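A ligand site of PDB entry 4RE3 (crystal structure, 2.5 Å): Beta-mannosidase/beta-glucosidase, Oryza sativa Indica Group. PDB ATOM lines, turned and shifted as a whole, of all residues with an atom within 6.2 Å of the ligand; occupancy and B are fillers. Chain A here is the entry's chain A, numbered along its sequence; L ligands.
The indole nitrogen (NE1) of Trp 464 sits at hydrogen-bond distance from an oxygen (O1) of the ligand (3.1 Å).
O2 of the ligand lies within hydrogen-bond range of OE2 of Glu 409 (2.6 Å).
The side-chain carboxylate (OE1) of Glu 463 sits at hydrogen-bond distance from an oxygen (O3) of the ligand.
NE2 of His 153 is in hydrogen-bond range of O1 of the ligand (2.8 Å).
The indole nitrogen (NE1) of Trp 456 sits close to an oxygen (O3) of the ligand (3.3 Å).
N2 of the ligand sits at hydrogen-bond distance from OE2 of Glu 199 (2.7 Å).
An oxygen (O1) of the ligand sits at hydrogen-bond distance from the side-chain amide oxygen of Gln 52, at 2.6 Å.
The side-chain amide nitrogen (ND2) of Asn 198 lies within hydrogen-bond range of an oxygen (O2) of the ligand, at 3.0 Å.
NE2 of His 153 sits close to ND2 of Asn 198 (3.2 Å).
The side-chain carboxylate (OE1) of Glu 199 lies within hydrogen-bond range of the side-chain sulfur (SG) of Cys 202 (3.8 Å).
The side-chain carboxylate of Glu 199 sits at hydrogen-bond distance from the side-chain hydroxyl of Tyr 154, at 2.6 Å.
OE1 of Gln 52 lies close to NE1 of Trp 464, at 3.2 Å.
ND2 of Asn 336 is in hydrogen-bond range of OE2 of Glu 199 (2.7 Å).
The side-chain amide oxygen (OE1) of Gln 52 sits at hydrogen-bond distance from the side-chain hydroxyl (OG) of Ser 49, 2.7 Å away.
OE2 of Glu 409 sits close to OD1 of Asn 198, 3.2 Å away.
The side-chain amide nitrogen (NE2) of Gln 52 is in hydrogen-bond range of the backbone carbonyl oxygen (O) of Phe 462.
OH of Tyr 338 sits close to N1 of the ligand.
Tyr 154 touches the ligand.
Trp 381 touches the ligand (CZ2 to O4, 3.3 Å).
Phe 472 touches the ligand (CZ to C6, 3.4 Å).
Hydrophobic or aromatic side chains within 4 Å of the ligand: His 153, Tyr 338, Trp 381, Trp 456, Trp 464 and Phe 472.
Within 4 Å of the ligand: Gln 52, His 153, Tyr 154, Asn 198, Glu 199, Tyr 338, Trp 381, Glu 409, Trp 456, Glu 463, Trp 464 and Phe 472.
The nearest printed residue that does not touch the ligand is Asn 336 (4.2 Å).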
ATOM      1  N   SER A  49      14.226  -7.959  25.580  1.00  0.00           N
ATOM      2  CA  SER A  49      13.392  -7.028  24.838  1.00  0.00           C
ATOM      3  C   SER A  49      12.163  -6.634  25.650  1.00  0.00           C
ATOM      4  O   SER A  49      11.680  -7.401  26.496  1.00  0.00           O
ATOM      5  CB  SER A  49      12.963  -7.638  23.508  1.00  0.00           C
ATOM      6  OG  SER A  49      11.856  -8.510  23.677  1.00  0.00           O
ATOM      7  N   GLN A  52       9.116  -9.113  25.619  1.00  0.00           N
ATOM      8  CA  GLN A  52       9.384 -10.436  26.134  1.00  0.00           C
ATOM      9  C   GLN A  52       9.503 -10.475  27.654  1.00  0.00           C
ATOM     10  O   GLN A  52       9.277 -11.513  28.243  1.00  0.00           O
ATOM     11  CB  GLN A  52      10.605 -11.031  25.450  1.00  0.00           C
ATOM     12  CG  GLN A  52      10.360 -11.274  23.967  1.00  0.00           C
ATOM     13  CD  GLN A  52      11.584 -11.798  23.250  1.00  0.00           C
ATOM     14  OE1 GLN A  52      12.372 -11.018  22.719  1.00  0.00           O
ATOM     15  NE2 GLN A  52      11.752 -13.113  23.235  1.00  0.00           N
ATOM     16  N   ARG A 109      21.502  -5.102  27.661  1.00  0.00           N
ATOM     17  CA  ARG A 109      20.863  -4.587  26.461  1.00  0.00           C
ATOM     18  C   ARG A 109      19.371  -4.853  26.576  1.00  0.00           C
ATOM     19  O   ARG A 109      18.930  -6.002  26.560  1.00  0.00           O
ATOM     20  CB  ARG A 109      21.465  -5.202  25.188  1.00  0.00           C
ATOM     21  CG  ARG A 109      20.871  -4.625  23.889  1.00  0.00           C
ATOM     22  CD  ARG A 109      19.786  -5.505  23.262  1.00  0.00           C
ATOM     23  NE  ARG A 109      20.361  -6.678  22.602  1.00  0.00           N
ATOM     24  CZ  ARG A 109      19.703  -7.487  21.762  1.00  0.00           C
ATOM     25  NH1 ARG A 109      18.436  -7.255  21.450  1.00  0.00           N
ATOM     26  NH2 ARG A 109      20.322  -8.536  21.238  1.00  0.00           N
ATOM     27  N   HIS A 153      12.107  -3.766  18.857  1.00  0.00           N
ATOM     28  CA  HIS A 153      12.206  -5.210  18.929  1.00  0.00           C
ATOM     29  C   HIS A 153      10.851  -5.865  18.665  1.00  0.00           C
ATOM     30  O   HIS A 153      10.201  -6.393  19.569  1.00  0.00           O
ATOM     31  CB  HIS A 153      12.834  -5.637  20.255  1.00  0.00           C
ATOM     32  CG  HIS A 153      13.358  -7.047  20.241  1.00  0.00           C
ATOM     33  ND1 HIS A 153      14.565  -7.382  20.811  1.00  0.00           N
ATOM     34  CD2 HIS A 153      12.844  -8.192  19.749  1.00  0.00           C
ATOM     35  CE1 HIS A 153      14.768  -8.678  20.668  1.00  0.00           C
ATOM     36  NE2 HIS A 153      13.735  -9.199  20.020  1.00  0.00           N
ATOM     37  N   TYR A 154      10.470  -5.812  17.392  1.00  0.00           N
ATOM     38  CA  TYR A 154       9.279  -6.435  16.798  1.00  0.00           C
ATOM     39  C   TYR A 154       7.950  -5.748  17.148  1.00  0.00           C
ATOM     40  O   TYR A 154       6.895  -6.253  16.751  1.00  0.00           O
ATOM     41  CB  TYR A 154       9.173  -7.940  17.098  1.00  0.00           C
ATOM     42  CG  TYR A 154      10.394  -8.791  16.803  1.00  0.00           C
ATOM     43  CD1 TYR A 154      10.473 -10.097  17.299  1.00  0.00           C
ATOM     44  CD2 TYR A 154      11.464  -8.310  16.040  1.00  0.00           C
ATOM     45  CE1 TYR A 154      11.559 -10.899  17.054  1.00  0.00           C
ATOM     46  CE2 TYR A 154      12.578  -9.132  15.773  1.00  0.00           C
ATOM     47  CZ  TYR A 154      12.612 -10.416  16.291  1.00  0.00           C
ATOM     48  OH  TYR A 154      13.697 -11.227  16.058  1.00  0.00           O
ATOM     49  N   ASN A 198      16.536  -4.308  16.413  1.00  0.00           N
ATOM     50  CA  ASN A 198      16.865  -5.708  16.541  1.00  0.00           C
ATOM     51  C   ASN A 198      16.385  -6.471  15.328  1.00  0.00           C
ATOM     52  O   ASN A 198      15.194  -6.584  15.090  1.00  0.00           O
ATOM     53  CB  ASN A 198      16.252  -6.342  17.785  1.00  0.00           C
ATOM     54  CG  ASN A 198      16.787  -7.734  18.036  1.00  0.00           C
ATOM     55  OD1 ASN A 198      17.933  -7.913  18.488  1.00  0.00           O
ATOM     56  ND2 ASN A 198      15.975  -8.746  17.710  1.00  0.00           N
ATOM     57  N   GLU A 199      17.338  -6.995  14.569  1.00  0.00           N
ATOM     58  CA  GLU A 199      17.055  -7.939  13.488  1.00  0.00           C
ATOM     59  C   GLU A 199      15.992  -7.473  12.492  1.00  0.00           C
ATOM     60  O   GLU A 199      14.917  -8.077  12.387  1.00  0.00           O
ATOM     61  CB  GLU A 199      16.707  -9.295  14.067  1.00  0.00           C
ATOM     62  CG  GLU A 199      17.783  -9.839  14.964  1.00  0.00           C
ATOM     63  CD  GLU A 199      17.404 -11.138  15.614  1.00  0.00           C
ATOM     64  OE1 GLU A 199      16.216 -11.549  15.545  1.00  0.00           O
ATOM     65  OE2 GLU A 199      18.311 -11.764  16.211  1.00  0.00           O
ATOM     66  N   CYS A 202      14.438 -10.208  10.330  1.00  0.00           N
ATOM     67  CA  CYS A 202      13.287 -10.973  10.821  1.00  0.00           C
ATOM     68  C   CYS A 202      12.009 -10.138  10.784  1.00  0.00           C
ATOM     69  O   CYS A 202      10.947 -10.640  10.416  1.00  0.00           O
ATOM     70  CB  CYS A 202      13.534 -11.572  12.207  1.00  0.00           C
ATOM     71  SG  CYS A 202      14.978 -12.707  12.173  1.00  0.00           S
ATOM     72  N   ASP A 266      20.939 -10.233  12.692  1.00  0.00           N
ATOM     73  CA  ASP A 266      21.112 -11.672  12.814  1.00  0.00           C
ATOM     74  C   ASP A 266      21.912 -12.210  11.638  1.00  0.00           C
ATOM     75  O   ASP A 266      21.810 -11.702  10.525  1.00  0.00           O
ATOM     76  CB  ASP A 266      19.783 -12.405  12.941  1.00  0.00           C
ATOM     77  CG  ASP A 266      18.860 -12.130  11.794  1.00  0.00           C
ATOM     78  OD1 ASP A 266      18.516 -10.932  11.590  1.00  0.00           O
ATOM     79  OD2 ASP A 266      18.488 -13.096  11.108  1.00  0.00           O
ATOM     80  N   ASN A 336      23.976 -10.882  16.024  1.00  0.00           N
ATOM     81  CA  ASN A 336      23.233 -11.860  16.830  1.00  0.00           C
ATOM     82  C   ASN A 336      23.487 -13.191  16.195  1.00  0.00           C
ATOM     83  O   ASN A 336      23.013 -13.421  15.072  1.00  0.00           O
ATOM     84  CB  ASN A 336      21.730 -11.595  16.765  1.00  0.00           C
ATOM     85  CG  ASN A 336      21.314 -10.297  17.437  1.00  0.00           C
ATOM     86  OD1 ASN A 336      22.146  -9.607  18.024  1.00  0.00           O
ATOM     87  ND2 ASN A 336      20.021  -9.980  17.357  1.00  0.00           N
ATOM     88  N   TYR A 338      23.621 -17.536  16.575  1.00  0.00           N
ATOM     89  CA  TYR A 338      23.221 -18.749  17.284  1.00  0.00           C
ATOM     90  C   TYR A 338      23.673 -20.038  16.616  1.00  0.00           C
ATOM     91  O   TYR A 338      24.076 -20.985  17.292  1.00  0.00           O
ATOM     92  CB  TYR A 338      21.709 -18.792  17.369  1.00  0.00           C
ATOM     93  CG  TYR A 338      21.109 -17.812  18.326  1.00  0.00           C
ATOM     94  CD1 TYR A 338      20.930 -16.488  17.961  1.00  0.00           C
ATOM     95  CD2 TYR A 338      20.689 -18.214  19.610  1.00  0.00           C
ATOM     96  CE1 TYR A 338      20.384 -15.573  18.843  1.00  0.00           C
ATOM     97  CE2 TYR A 338      20.131 -17.300  20.500  1.00  0.00           C
ATOM     98  CZ  TYR A 338      19.969 -15.993  20.095  1.00  0.00           C
ATOM     99  OH  TYR A 338      19.418 -15.077  20.932  1.00  0.00           O
ATOM    100  N   SER A 379      14.449 -25.099  20.223  1.00  0.00           N
ATOM    101  CA  SER A 379      13.907 -24.436  19.020  1.00  0.00           C
ATOM    102  C   SER A 379      14.269 -25.225  17.777  1.00  0.00           C
ATOM    103  O   SER A 379      15.391 -25.722  17.668  1.00  0.00           O
ATOM    104  CB  SER A 379      14.470 -23.020  18.876  1.00  0.00           C
ATOM    105  OG  SER A 379      13.927 -22.158  19.853  1.00  0.00           O
ATOM    106  N   TRP A 381      15.094 -24.380  14.863  1.00  0.00           N
ATOM    107  CA  TRP A 381      16.114 -23.799  14.011  1.00  0.00           C
ATOM    108  C   TRP A 381      17.491 -23.782  14.653  1.00  0.00           C
ATOM    109  O   TRP A 381      18.494 -23.456  13.994  1.00  0.00           O
ATOM    110  CB  TRP A 381      15.721 -22.358  13.643  1.00  0.00           C
ATOM    111  CG  TRP A 381      15.446 -21.537  14.813  1.00  0.00           C
ATOM    112  CD1 TRP A 381      14.250 -21.417  15.438  1.00  0.00           C
ATOM    113  CD2 TRP A 381      16.372 -20.752  15.545  1.00  0.00           C
ATOM    114  NE1 TRP A 381      14.363 -20.580  16.530  1.00  0.00           N
ATOM    115  CE2 TRP A 381      15.663 -20.155  16.615  1.00  0.00           C
ATOM    116  CE3 TRP A 381      17.733 -20.468  15.410  1.00  0.00           C
ATOM    117  CZ2 TRP A 381      16.272 -19.297  17.535  1.00  0.00           C
ATOM    118  CZ3 TRP A 381      18.336 -19.609  16.322  1.00  0.00           C
ATOM    119  CH2 TRP A 381      17.607 -19.043  17.373  1.00  0.00           C
ATOM    120  N   LEU A 382      17.556 -24.114  15.943  1.00  0.00           N
ATOM    121  CA  LEU A 382      18.799 -23.919  16.678  1.00  0.00           C
ATOM    122  C   LEU A 382      19.616 -25.184  16.728  1.00  0.00           C
ATOM    123  O   LEU A 382      19.293 -26.120  17.454  1.00  0.00           O
ATOM    124  CB  LEU A 382      18.529 -23.409  18.099  1.00  0.00           C
ATOM    125  CG  LEU A 382      19.546 -22.421  18.687  1.00  0.00           C
ATOM    126  CD1 LEU A 382      18.972 -21.803  19.966  1.00  0.00           C
ATOM    127  CD2 LEU A 382      20.923 -23.038  18.944  1.00  0.00           C
ATOM    128  N   GLU A 409      23.917 -11.166  20.682  1.00  0.00           N
ATOM    129  CA  GLU A 409      23.016 -12.239  21.178  1.00  0.00           C
ATOM    130  C   GLU A 409      23.596 -13.583  20.876  1.00  0.00           C
ATOM    131  O   GLU A 409      24.167 -13.804  19.805  1.00  0.00           O
ATOM    132  CB  GLU A 409      21.638 -12.213  20.499  1.00  0.00           C
ATOM    133  CG  GLU A 409      20.543 -11.560  21.273  1.00  0.00           C
ATOM    134  CD  GLU A 409      19.224 -11.606  20.514  1.00  0.00           C
ATOM    135  OE1 GLU A 409      18.743 -12.723  20.177  1.00  0.00           O
ATOM    136  OE2 GLU A 409      18.642 -10.527  20.265  1.00  0.00           O
ATOM    137  N   TRP A 456      21.781 -14.048  25.282  1.00  0.00           N
ATOM    138  CA  TRP A 456      20.324 -14.122  25.348  1.00  0.00           C
ATOM    139  C   TRP A 456      19.943 -15.404  26.149  1.00  0.00           C
ATOM    140  O   TRP A 456      20.279 -16.515  25.734  1.00  0.00           O
ATOM    141  CB  TRP A 456      19.688 -14.144  23.954  1.00  0.00           C
ATOM    142  CG  TRP A 456      18.204 -14.039  24.045  1.00  0.00           C
ATOM    143  CD1 TRP A 456      17.315 -15.052  24.354  1.00  0.00           C
ATOM    144  CD2 TRP A 456      17.399 -12.852  23.896  1.00  0.00           C
ATOM    145  NE1 TRP A 456      16.038 -14.557  24.404  1.00  0.00           N
ATOM    146  CE2 TRP A 456      16.056 -13.213  24.135  1.00  0.00           C
ATOM    147  CE3 TRP A 456      17.696 -11.517  23.588  1.00  0.00           C
ATOM    148  CZ2 TRP A 456      15.002 -12.308  24.054  1.00  0.00           C
ATOM    149  CZ3 TRP A 456      16.649 -10.605  23.505  1.00  0.00           C
ATOM    150  CH2 TRP A 456      15.325 -11.002  23.735  1.00  0.00           C
ATOM    151  N   ASN A 461      11.685 -16.264  29.199  1.00  0.00           N
ATOM    152  CA  ASN A 461      10.704 -15.232  28.882  1.00  0.00           C
ATOM    153  C   ASN A 461       9.742 -15.618  27.747  1.00  0.00           C
ATOM    154  O   ASN A 461       9.756 -16.771  27.275  1.00  0.00           O
ATOM    155  CB  ASN A 461      11.392 -13.871  28.644  1.00  0.00           C
ATOM    156  CG  ASN A 461      12.459 -13.916  27.548  1.00  0.00           C
ATOM    157  OD1 ASN A 461      12.204 -14.372  26.422  1.00  0.00           O
ATOM    158  ND2 ASN A 461      13.649 -13.431  27.853  1.00  0.00           N
ATOM    159  N   PHE A 462       8.886 -14.693  27.348  1.00  0.00           N
ATOM    160  CA  PHE A 462       7.939 -14.931  26.263  1.00  0.00           C
ATOM    161  C   PHE A 462       8.700 -15.123  24.953  1.00  0.00           C
ATOM    162  O   PHE A 462       9.312 -14.196  24.439  1.00  0.00           O
ATOM    163  CB  PHE A 462       6.938 -13.763  26.175  1.00  0.00           C
ATOM    164  CG  PHE A 462       5.941 -13.881  25.054  1.00  0.00           C
ATOM    165  CD1 PHE A 462       4.886 -14.779  25.134  1.00  0.00           C
ATOM    166  CD2 PHE A 462       6.053 -13.068  23.924  1.00  0.00           C
ATOM    167  CE1 PHE A 462       3.962 -14.891  24.100  1.00  0.00           C
ATOM    168  CE2 PHE A 462       5.132 -13.158  22.883  1.00  0.00           C
ATOM    169  CZ  PHE A 462       4.086 -14.078  22.963  1.00  0.00           C
ATOM    170  N   GLU A 463       8.652 -16.330  24.412  1.00  0.00           N
ATOM    171  CA  GLU A 463       9.419 -16.643  23.214  1.00  0.00           C
ATOM    172  C   GLU A 463       8.570 -16.518  21.934  1.00  0.00           C
ATOM    173  O   GLU A 463       8.423 -17.478  21.152  1.00  0.00           O
ATOM    174  CB  GLU A 463      10.091 -18.032  23.365  1.00  0.00           C
ATOM    175  CG  GLU A 463      11.032 -18.451  22.212  1.00  0.00           C
ATOM    176  CD  GLU A 463      12.046 -17.383  21.799  1.00  0.00           C
ATOM    177  OE1 GLU A 463      12.448 -16.531  22.634  1.00  0.00           O
ATOM    178  OE2 GLU A 463      12.480 -17.402  20.610  1.00  0.00           O
ATOM    179  N   TRP A 464       8.007 -15.316  21.716  1.00  0.00           N
ATOM    180  CA  TRP A 464       7.224 -15.054  20.475  1.00  0.00           C
ATOM    181  C   TRP A 464       6.252 -16.195  20.161  1.00  0.00           C
ATOM    182  O   TRP A 464       5.440 -16.578  21.035  1.00  0.00           O
ATOM    183  CB  TRP A 464       8.152 -14.709  19.297  1.00  0.00           C
ATOM    184  CG  TRP A 464       9.038 -13.544  19.649  1.00  0.00           C
ATOM    185  CD1 TRP A 464      10.398 -13.555  19.796  1.00  0.00           C
ATOM    186  CD2 TRP A 464       8.612 -12.216  19.993  1.00  0.00           C
ATOM    187  NE1 TRP A 464      10.857 -12.309  20.152  1.00  0.00           N
ATOM    188  CE2 TRP A 464       9.773 -11.461  20.297  1.00  0.00           C
ATOM    189  CE3 TRP A 464       7.362 -11.579  20.036  1.00  0.00           C
ATOM    190  CZ2 TRP A 464       9.722 -10.102  20.648  1.00  0.00           C
ATOM    191  CZ3 TRP A 464       7.304 -10.227  20.390  1.00  0.00           C
ATOM    192  CH2 TRP A 464       8.480  -9.502  20.689  1.00  0.00           C
ATOM    193  N   PHE A 472      15.007 -19.859  27.344  1.00  0.00           N
ATOM    194  CA  PHE A 472      16.327 -19.405  26.875  1.00  0.00           C
ATOM    195  C   PHE A 472      17.193 -18.794  27.981  1.00  0.00           C
ATOM    196  O   PHE A 472      18.326 -18.394  27.730  1.00  0.00           O
ATOM    197  CB  PHE A 472      16.146 -18.328  25.817  1.00  0.00           C
ATOM    198  CG  PHE A 472      16.089 -18.850  24.412  1.00  0.00           C
ATOM    199  CD1 PHE A 472      17.257 -19.094  23.689  1.00  0.00           C
ATOM    200  CD2 PHE A 472      14.845 -19.072  23.792  1.00  0.00           C
ATOM    201  CE1 PHE A 472      17.204 -19.549  22.396  1.00  0.00           C
ATOM    202  CE2 PHE A 472      14.774 -19.530  22.484  1.00  0.00           C
ATOM    203  CZ  PHE A 472      15.965 -19.773  21.784  1.00  0.00           C
HETATM  204  C1  LIG L   1      16.301 -13.636  18.575  1.00  0.00           C
HETATM  205  C2  LIG L   1      15.541 -12.450  19.066  1.00  0.00           C
HETATM  206  N1  LIG L   1      16.449 -14.791  19.233  1.00  0.00           N
HETATM  207  C3  LIG L   1      14.973 -12.741  20.461  1.00  0.00           C
HETATM  208  C4  LIG L   1      14.590 -14.203  20.635  1.00  0.00           C
HETATM  209  C5  LIG L   1      15.859 -15.035  20.581  1.00  0.00           C
HETATM  210  C6  LIG L   1      15.678 -16.541  20.844  1.00  0.00           C
HETATM  211  C7  LIG L   1      17.508 -14.976  17.329  1.00  0.00           C
HETATM  212  C8  LIG L   1      17.175 -15.625  18.484  1.00  0.00           C
HETATM  213  N2  LIG L   1      16.962 -13.754  17.397  1.00  0.00           N
HETATM  214  O1  LIG L   1      13.852 -11.887  20.716  1.00  0.00           O
HETATM  215  O2  LIG L   1      16.404 -11.303  19.123  1.00  0.00           O
HETATM  216  O3  LIG L   1      13.874 -14.413  21.866  1.00  0.00           O
HETATM  217  O4  LIG L   1      15.025 -17.220  19.753  1.00  0.00           O
